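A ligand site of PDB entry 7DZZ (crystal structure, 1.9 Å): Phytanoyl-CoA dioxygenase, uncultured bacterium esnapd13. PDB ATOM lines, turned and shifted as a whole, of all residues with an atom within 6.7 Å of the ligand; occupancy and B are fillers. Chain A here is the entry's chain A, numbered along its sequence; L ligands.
NH1 of Arg 248 is in hydrogen-bond range of OG1 of Thr 174, at 3.1 Å. The side-chain carboxylate (OD2) of Asp 126 is in salt-bridge range of the guanidinium group (NH2) of Arg 248, at 2.7 Å. OG1 of Thr 174 sits at hydrogen-bond distance from O of Trp 171 (2.6 Å). NE1 of Trp 122 sits at hydrogen-bond distance from OE1 of Gln 99 (3.5 Å). The side-chain amide oxygen (OE1) of Gln 99 is in hydrogen-bond range of the side-chain amino group (NZ) of Lys 101, 2.8 Å away. NE2 of Gln 99 sits at hydrogen-bond distance from O of Leu 252 (2.9 Å). NE2 of His 116 sits at hydrogen-bond distance from OD1 of Asp 118 (3.2 Å). The backbone carbonyl oxygen (O) of His 116 is in hydrogen-bond range of the backbone NH (N) of His 216 (2.8 Å).
Trp 113 touches the ligand. His 116 touches the ligand. Asp 118 touches the ligand (OD1 to C4, 3.5 Å). Phe 121 touches the ligand (CD2 to O2, 3.5 Å). CB of Leu 175 touches N1 of the ligand, at 3.9 Å. Of the 22 residues printed, 9 come within 4 Å of the ligand.
NH1 of Arg 248 lies within salt-bridge range of O2 of the ligand. O of Thr 174 sits at hydrogen-bond distance from N1 of the ligand, at 3.0 Å. An oxygen (O1) of the ligand is in hydrogen-bond range of the indole nitrogen of Trp 122. The side-chain amide nitrogen of Gln 99 is in hydrogen-bond range of an oxygen (O1) of the ligand, 3.2 Å away.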
ATOM      1  N   HIS A  65      -4.069  -0.911  -2.086  1.00  0.00           N
ATOM      2  CA  HIS A  65      -5.138  -1.235  -2.993  1.00  0.00           C
ATOM      3  C   HIS A  65      -6.062  -0.017  -3.305  1.00  0.00           C
ATOM      4  O   HIS A  65      -6.381   0.796  -2.434  1.00  0.00           O
ATOM      5  CB  HIS A  65      -5.956  -2.440  -2.461  1.00  0.00           C
ATOM      6  CG  HIS A  65      -5.176  -3.715  -2.300  1.00  0.00           C
ATOM      7  ND1 HIS A  65      -4.182  -3.876  -1.356  1.00  0.00           N
ATOM      8  CD2 HIS A  65      -5.230  -4.880  -2.999  1.00  0.00           C
ATOM      9  CE1 HIS A  65      -3.647  -5.077  -1.491  1.00  0.00           C
ATOM     10  NE2 HIS A  65      -4.275  -5.711  -2.468  1.00  0.00           N
ATOM     11  N   HIS A  98     -11.284  -3.007 -12.540  1.00  0.00           N
ATOM     12  CA  HIS A  98     -11.853  -3.899 -11.516  1.00  0.00           C
ATOM     13  C   HIS A  98     -11.067  -3.726 -10.204  1.00  0.00           C
ATOM     14  O   HIS A  98     -11.675  -3.614  -9.118  1.00  0.00           O
ATOM     15  CB  HIS A  98     -11.812  -5.358 -11.916  1.00  0.00           C
ATOM     16  CG  HIS A  98     -12.209  -6.319 -10.815  1.00  0.00           C
ATOM     17  ND1 HIS A  98     -13.436  -6.302 -10.230  1.00  0.00           N
ATOM     18  CD2 HIS A  98     -11.477  -7.234 -10.127  1.00  0.00           C
ATOM     19  CE1 HIS A  98     -13.473  -7.188  -9.242  1.00  0.00           C
ATOM     20  NE2 HIS A  98     -12.289  -7.763  -9.169  1.00  0.00           N
ATOM     21  N   GLN A  99      -9.748  -3.713 -10.339  1.00  0.00           N
ATOM     22  CA  GLN A  99      -8.853  -3.628  -9.156  1.00  0.00           C
ATOM     23  C   GLN A  99      -7.551  -2.922  -9.557  1.00  0.00           C
ATOM     24  O   GLN A  99      -7.105  -2.991 -10.705  1.00  0.00           O
ATOM     25  CB  GLN A  99      -8.622  -5.053  -8.597  1.00  0.00           C
ATOM     26  CG  GLN A  99      -7.517  -5.268  -7.533  1.00  0.00           C
ATOM     27  CD  GLN A  99      -7.521  -6.720  -7.058  1.00  0.00           C
ATOM     28  OE1 GLN A  99      -6.747  -7.573  -7.563  1.00  0.00           O
ATOM     29  NE2 GLN A  99      -8.527  -7.039  -6.216  1.00  0.00           N
ATOM     30  N   LYS A 101      -3.670  -2.151  -7.644  1.00  0.00           N
ATOM     31  CA  LYS A 101      -2.810  -2.373  -6.457  1.00  0.00           C
ATOM     32  C   LYS A 101      -1.386  -2.134  -6.793  1.00  0.00           C
ATOM     33  O   LYS A 101      -0.937  -2.325  -7.949  1.00  0.00           O
ATOM     34  CB  LYS A 101      -2.946  -3.777  -5.931  1.00  0.00           C
ATOM     35  CG  LYS A 101      -2.703  -4.901  -6.890  1.00  0.00           C
ATOM     36  CD  LYS A 101      -3.172  -6.278  -6.327  1.00  0.00           C
ATOM     37  CE  LYS A 101      -3.052  -7.396  -7.394  1.00  0.00           C
ATOM     38  NZ  LYS A 101      -4.136  -7.390  -8.441  1.00  0.00           N
ATOM     39  N   ASN A 103       2.212  -3.460  -5.420  1.00  0.00           N
ATOM     40  CA  ASN A 103       2.853  -4.523  -4.672  1.00  0.00           C
ATOM     41  C   ASN A 103       4.341  -4.186  -4.698  1.00  0.00           C
ATOM     42  O   ASN A 103       5.018  -4.338  -5.741  1.00  0.00           O
ATOM     43  CB  ASN A 103       2.601  -5.909  -5.299  1.00  0.00           C
ATOM     44  CG  ASN A 103       1.208  -6.498  -4.976  1.00  0.00           C
ATOM     45  OD1 ASN A 103       0.455  -6.013  -4.112  1.00  0.00           O
ATOM     46  ND2 ASN A 103       0.875  -7.572  -5.661  1.00  0.00           N
ATOM     47  N   TRP A 113       4.320 -14.642  -3.146  1.00  0.00           N
ATOM     48  CA  TRP A 113       2.914 -14.768  -3.574  1.00  0.00           C
ATOM     49  C   TRP A 113       2.809 -16.216  -4.028  1.00  0.00           C
ATOM     50  O   TRP A 113       3.414 -16.564  -5.049  1.00  0.00           O
ATOM     51  CB  TRP A 113       2.555 -13.768  -4.739  1.00  0.00           C
ATOM     52  CG  TRP A 113       2.334 -12.304  -4.248  1.00  0.00           C
ATOM     53  CD1 TRP A 113       3.275 -11.284  -4.193  1.00  0.00           C
ATOM     54  CD2 TRP A 113       1.110 -11.738  -3.705  1.00  0.00           C
ATOM     55  NE1 TRP A 113       2.715 -10.140  -3.651  1.00  0.00           N
ATOM     56  CE2 TRP A 113       1.391 -10.380  -3.354  1.00  0.00           C
ATOM     57  CE3 TRP A 113      -0.185 -12.242  -3.492  1.00  0.00           C
ATOM     58  CZ2 TRP A 113       0.403  -9.518  -2.775  1.00  0.00           C
ATOM     59  CZ3 TRP A 113      -1.175 -11.374  -2.919  1.00  0.00           C
ATOM     60  CH2 TRP A 113      -0.865 -10.047  -2.564  1.00  0.00           C
ATOM     61  N   HIS A 116      -1.516 -18.823  -7.955  1.00  0.00           N
ATOM     62  CA  HIS A 116      -2.928 -18.489  -8.040  1.00  0.00           C
ATOM     63  C   HIS A 116      -3.284 -18.045  -9.443  1.00  0.00           C
ATOM     64  O   HIS A 116      -2.414 -17.774 -10.299  1.00  0.00           O
ATOM     65  CB  HIS A 116      -3.353 -17.469  -7.011  1.00  0.00           C
ATOM     66  CG  HIS A 116      -2.769 -16.102  -7.225  1.00  0.00           C
ATOM     67  ND1 HIS A 116      -1.427 -15.817  -7.024  1.00  0.00           N
ATOM     68  CD2 HIS A 116      -3.345 -14.946  -7.625  1.00  0.00           C
ATOM     69  CE1 HIS A 116      -1.208 -14.552  -7.308  1.00  0.00           C
ATOM     70  NE2 HIS A 116      -2.346 -14.002  -7.674  1.00  0.00           N
ATOM     71  N   GLN A 117      -4.576 -18.115  -9.700  1.00  0.00           N
ATOM     72  CA  GLN A 117      -5.241 -17.491 -10.878  1.00  0.00           C
ATOM     73  C   GLN A 117      -6.119 -16.384 -10.267  1.00  0.00           C
ATOM     74  O   GLN A 117      -6.989 -16.629  -9.386  1.00  0.00           O
ATOM     75  CB  GLN A 117      -6.067 -18.535 -11.600  1.00  0.00           C
ATOM     76  CG  GLN A 117      -5.259 -19.552 -12.404  1.00  0.00           C
ATOM     77  CD  GLN A 117      -6.153 -20.718 -12.931  1.00  0.00           C
ATOM     78  OE1 GLN A 117      -6.813 -21.345 -12.135  1.00  0.00           O
ATOM     79  NE2 GLN A 117      -6.121 -21.020 -14.238  1.00  0.00           N
ATOM     80  N   ASP A 118      -5.881 -15.146 -10.697  1.00  0.00           N
ATOM     81  CA  ASP A 118      -6.670 -14.007 -10.220  1.00  0.00           C
ATOM     82  C   ASP A 118      -8.159 -14.288 -10.425  1.00  0.00           C
ATOM     83  O   ASP A 118      -8.952 -13.901  -9.591  1.00  0.00           O
ATOM     84  CB  ASP A 118      -6.329 -12.681 -10.988  1.00  0.00           C
ATOM     85  CG  ASP A 118      -4.889 -12.164 -10.738  1.00  0.00           C
ATOM     86  OD1 ASP A 118      -4.376 -12.420  -9.615  1.00  0.00           O
ATOM     87  OD2 ASP A 118      -4.296 -11.475 -11.655  1.00  0.00           O
ATOM     88  N   PHE A 121     -10.208 -15.832  -7.616  1.00  0.00           N
ATOM     89  CA  PHE A 121     -10.546 -14.900  -6.581  1.00  0.00           C
ATOM     90  C   PHE A 121     -11.712 -14.034  -7.026  1.00  0.00           C
ATOM     91  O   PHE A 121     -12.665 -13.793  -6.285  1.00  0.00           O
ATOM     92  CB  PHE A 121      -9.398 -13.913  -6.265  1.00  0.00           C
ATOM     93  CG  PHE A 121      -8.271 -14.494  -5.470  1.00  0.00           C
ATOM     94  CD1 PHE A 121      -7.389 -15.418  -6.057  1.00  0.00           C
ATOM     95  CD2 PHE A 121      -8.094 -14.117  -4.125  1.00  0.00           C
ATOM     96  CE1 PHE A 121      -6.354 -15.980  -5.308  1.00  0.00           C
ATOM     97  CE2 PHE A 121      -7.057 -14.671  -3.396  1.00  0.00           C
ATOM     98  CZ  PHE A 121      -6.183 -15.600  -3.986  1.00  0.00           C
ATOM     99  N   TRP A 122     -11.592 -13.492  -8.219  1.00  0.00           N
ATOM    100  CA  TRP A 122     -12.587 -12.476  -8.642  1.00  0.00           C
ATOM    101  C   TRP A 122     -13.979 -13.070  -8.866  1.00  0.00           C
ATOM    102  O   TRP A 122     -14.977 -12.445  -8.548  1.00  0.00           O
ATOM    103  CB  TRP A 122     -12.077 -11.708  -9.875  1.00  0.00           C
ATOM    104  CG  TRP A 122     -10.806 -10.970  -9.623  1.00  0.00           C
ATOM    105  CD1 TRP A 122     -10.402 -10.434  -8.431  1.00  0.00           C
ATOM    106  CD2 TRP A 122      -9.781 -10.668 -10.557  1.00  0.00           C
ATOM    107  NE1 TRP A 122      -9.203  -9.852  -8.573  1.00  0.00           N
ATOM    108  CE2 TRP A 122      -8.797  -9.951  -9.869  1.00  0.00           C
ATOM    109  CE3 TRP A 122      -9.634 -10.871 -11.909  1.00  0.00           C
ATOM    110  CZ2 TRP A 122      -7.655  -9.437 -10.493  1.00  0.00           C
ATOM    111  CZ3 TRP A 122      -8.465 -10.375 -12.543  1.00  0.00           C
ATOM    112  CH2 TRP A 122      -7.495  -9.697 -11.819  1.00  0.00           C
ATOM    113  N   GLU A 125     -14.940 -14.237  -4.917  1.00  0.00           N
ATOM    114  CA  GLU A 125     -15.128 -13.123  -3.995  1.00  0.00           C
ATOM    115  C   GLU A 125     -16.030 -12.040  -4.518  1.00  0.00           C
ATOM    116  O   GLU A 125     -16.707 -11.364  -3.712  1.00  0.00           O
ATOM    117  CB  GLU A 125     -13.807 -12.466  -3.606  1.00  0.00           C
ATOM    118  CG  GLU A 125     -12.762 -13.380  -2.979  1.00  0.00           C
ATOM    119  CD  GLU A 125     -13.149 -13.791  -1.563  1.00  0.00           C
ATOM    120  OE1 GLU A 125     -13.217 -12.887  -0.693  1.00  0.00           O
ATOM    121  OE2 GLU A 125     -13.431 -14.989  -1.354  1.00  0.00           O
ATOM    122  N   ASP A 126     -15.971 -11.776  -5.828  1.00  0.00           N
ATOM    123  CA  ASP A 126     -16.572 -10.517  -6.363  1.00  0.00           C
ATOM    124  C   ASP A 126     -17.675 -10.741  -7.347  1.00  0.00           C
ATOM    125  O   ASP A 126     -18.306  -9.796  -7.715  1.00  0.00           O
ATOM    126  CB  ASP A 126     -15.530  -9.596  -7.016  1.00  0.00           C
ATOM    127  CG  ASP A 126     -14.368  -9.323  -6.112  1.00  0.00           C
ATOM    128  OD1 ASP A 126     -14.588  -9.013  -4.908  1.00  0.00           O
ATOM    129  OD2 ASP A 126     -13.216  -9.431  -6.641  1.00  0.00           O
ATOM    130  N   TRP A 171     -12.556 -11.978   3.765  1.00  0.00           N
ATOM    131  CA  TRP A 171     -11.724 -11.552   2.615  1.00  0.00           C
ATOM    132  C   TRP A 171     -10.283 -11.210   2.991  1.00  0.00           C
ATOM    133  O   TRP A 171      -9.444 -11.106   2.091  1.00  0.00           O
ATOM    134  CB  TRP A 171     -12.362 -10.406   1.819  1.00  0.00           C
ATOM    135  CG  TRP A 171     -12.753  -9.140   2.541  1.00  0.00           C
ATOM    136  CD1 TRP A 171     -14.029  -8.765   2.936  1.00  0.00           C
ATOM    137  CD2 TRP A 171     -11.903  -8.055   2.883  1.00  0.00           C
ATOM    138  NE1 TRP A 171     -13.994  -7.524   3.558  1.00  0.00           N
ATOM    139  CE2 TRP A 171     -12.701  -7.063   3.531  1.00  0.00           C
ATOM    140  CE3 TRP A 171     -10.529  -7.830   2.745  1.00  0.00           C
ATOM    141  CZ2 TRP A 171     -12.174  -5.875   4.025  1.00  0.00           C
ATOM    142  CZ3 TRP A 171      -9.994  -6.654   3.240  1.00  0.00           C
ATOM    143  CH2 TRP A 171     -10.820  -5.687   3.870  1.00  0.00           C
ATOM    144  N   ASN A 173      -7.590 -12.741   4.065  1.00  0.00           N
ATOM    145  CA  ASN A 173      -6.468 -13.553   3.574  1.00  0.00           C
ATOM    146  C   ASN A 173      -6.383 -13.645   2.004  1.00  0.00           C
ATOM    147  O   ASN A 173      -5.616 -14.471   1.471  1.00  0.00           O
ATOM    148  CB  ASN A 173      -6.484 -14.939   4.247  1.00  0.00           C
ATOM    149  CG  ASN A 173      -7.714 -15.804   3.886  1.00  0.00           C
ATOM    150  OD1 ASN A 173      -7.585 -16.782   3.142  1.00  0.00           O
ATOM    151  ND2 ASN A 173      -8.896 -15.459   4.443  1.00  0.00           N
ATOM    152  N   THR A 174      -7.128 -12.780   1.299  1.00  0.00           N
ATOM    153  CA  THR A 174      -7.085 -12.705  -0.195  1.00  0.00           C
ATOM    154  C   THR A 174      -5.767 -12.088  -0.802  1.00  0.00           C
ATOM    155  O   THR A 174      -5.390 -12.353  -1.942  1.00  0.00           O
ATOM    156  CB  THR A 174      -8.368 -12.003  -0.789  1.00  0.00           C
ATOM    157  OG1 THR A 174      -8.491 -10.640  -0.336  1.00  0.00           O
ATOM    158  CG2 THR A 174      -9.675 -12.796  -0.430  1.00  0.00           C
ATOM    159  N   LEU A 175      -5.040 -11.305  -0.015  1.00  0.00           N
ATOM    160  CA  LEU A 175      -3.864 -10.610  -0.525  1.00  0.00           C
ATOM    161  C   LEU A 175      -2.701 -10.735   0.499  1.00  0.00           C
ATOM    162  O   LEU A 175      -1.918  -9.794   0.686  1.00  0.00           O
ATOM    163  CB  LEU A 175      -4.239  -9.164  -0.915  1.00  0.00           C
ATOM    164  CG  LEU A 175      -5.201  -8.468   0.080  1.00  0.00           C
ATOM    165  CD1 LEU A 175      -4.425  -7.904   1.238  1.00  0.00           C
ATOM    166  CD2 LEU A 175      -6.091  -7.397  -0.529  1.00  0.00           C
ATOM    167  N   THR A 176      -2.594 -11.927   1.149  1.00  0.00           N
ATOM    168  CA  THR A 176      -1.463 -12.288   2.046  1.00  0.00           C
ATOM    169  C   THR A 176      -0.480 -13.295   1.381  1.00  0.00           C
ATOM    170  O   THR A 176      -0.681 -13.760   0.254  1.00  0.00           O
ATOM    171  CB  THR A 176      -1.938 -12.834   3.421  1.00  0.00           C
ATOM    172  OG1 THR A 176      -2.802 -13.953   3.248  1.00  0.00           O
ATOM    173  CG2 THR A 176      -2.661 -11.760   4.204  1.00  0.00           C
ATOM    174  N   LEU A 179      -2.382 -17.428   0.670  1.00  0.00           N
ATOM    175  CA  LEU A 179      -3.565 -17.112  -0.173  1.00  0.00           C
ATOM    176  C   LEU A 179      -4.811 -17.981   0.038  1.00  0.00           C
ATOM    177  O   LEU A 179      -4.715 -19.193   0.098  1.00  0.00           O
ATOM    178  CB  LEU A 179      -3.185 -17.289  -1.642  1.00  0.00           C
ATOM    179  CG  LEU A 179      -2.156 -16.305  -2.157  1.00  0.00           C
ATOM    180  CD1 LEU A 179      -1.806 -16.679  -3.585  1.00  0.00           C
ATOM    181  CD2 LEU A 179      -2.696 -14.888  -2.064  1.00  0.00           C
ATOM    182  N   HIS A 216      -0.032 -17.769 -11.714  1.00  0.00           N
ATOM    183  CA  HIS A 216       1.221 -17.077 -11.501  1.00  0.00           C
ATOM    184  C   HIS A 216       1.579 -17.025 -10.050  1.00  0.00           C
ATOM    185  O   HIS A 216       0.746 -17.291  -9.169  1.00  0.00           O
ATOM    186  CB  HIS A 216       1.206 -15.651 -12.156  1.00  0.00           C
ATOM    187  CG  HIS A 216       0.300 -14.704 -11.469  1.00  0.00           C
ATOM    188  ND1 HIS A 216      -1.061 -14.721 -11.657  1.00  0.00           N
ATOM    189  CD2 HIS A 216       0.553 -13.679 -10.613  1.00  0.00           C
ATOM    190  CE1 HIS A 216      -1.611 -13.746 -10.956  1.00  0.00           C
ATOM    191  NE2 HIS A 216      -0.651 -13.117 -10.293  1.00  0.00           N
ATOM    192  N   ARG A 248     -16.710  -7.554  -0.917  1.00  0.00           N
ATOM    193  CA  ARG A 248     -15.492  -6.788  -0.595  1.00  0.00           C
ATOM    194  C   ARG A 248     -15.695  -5.349  -0.804  1.00  0.00           C
ATOM    195  O   ARG A 248     -16.576  -4.974  -1.534  1.00  0.00           O
ATOM    196  CB  ARG A 248     -14.358  -7.254  -1.432  1.00  0.00           C
ATOM    197  CG  ARG A 248     -14.122  -8.726  -1.291  1.00  0.00           C
ATOM    198  CD  ARG A 248     -12.693  -9.073  -1.580  1.00  0.00           C
ATOM    199  NE  ARG A 248     -12.383  -9.044  -3.028  1.00  0.00           N
ATOM    200  CZ  ARG A 248     -11.234  -9.442  -3.572  1.00  0.00           C
ATOM    201  NH1 ARG A 248     -10.221  -9.810  -2.782  1.00  0.00           N
ATOM    202  NH2 ARG A 248     -11.068  -9.453  -4.924  1.00  0.00           N
ATOM    203  N   LEU A 252     -11.070  -2.932  -3.284  1.00  0.00           N
ATOM    204  CA  LEU A 252     -10.662  -4.206  -3.832  1.00  0.00           C
ATOM    205  C   LEU A 252     -11.459  -4.663  -5.079  1.00  0.00           C
ATOM    206  O   LEU A 252     -10.940  -5.398  -5.891  1.00  0.00           O
ATOM    207  CB  LEU A 252     -10.842  -5.287  -2.761  1.00  0.00           C
ATOM    208  CG  LEU A 252      -9.936  -5.072  -1.551  1.00  0.00           C
ATOM    209  CD1 LEU A 252     -10.308  -6.042  -0.437  1.00  0.00           C
ATOM    210  CD2 LEU A 252      -8.495  -5.318  -1.972  1.00  0.00           C
HETATM  211  N1  LIG L   1      -4.914 -10.776  -4.452  1.00  0.00           N
HETATM  212  C1  LIG L   1      -5.932 -10.259  -5.380  1.00  0.00           C
HETATM  213  C2  LIG L   1      -7.390 -10.399  -4.908  1.00  0.00           C
HETATM  214  O1  LIG L   1      -8.276 -10.159  -5.671  1.00  0.00           O
HETATM  215  C3  LIG L   1      -5.705 -11.053  -6.679  1.00  0.00           C
HETATM  216  C4  LIG L   1      -5.007 -12.283  -6.225  1.00  0.00           C
HETATM  217  C5  LIG L   1      -4.124 -11.854  -5.069  1.00  0.00           C
HETATM  218  O2  LIG L   1      -7.769 -10.676  -3.776  1.00  0.00           O
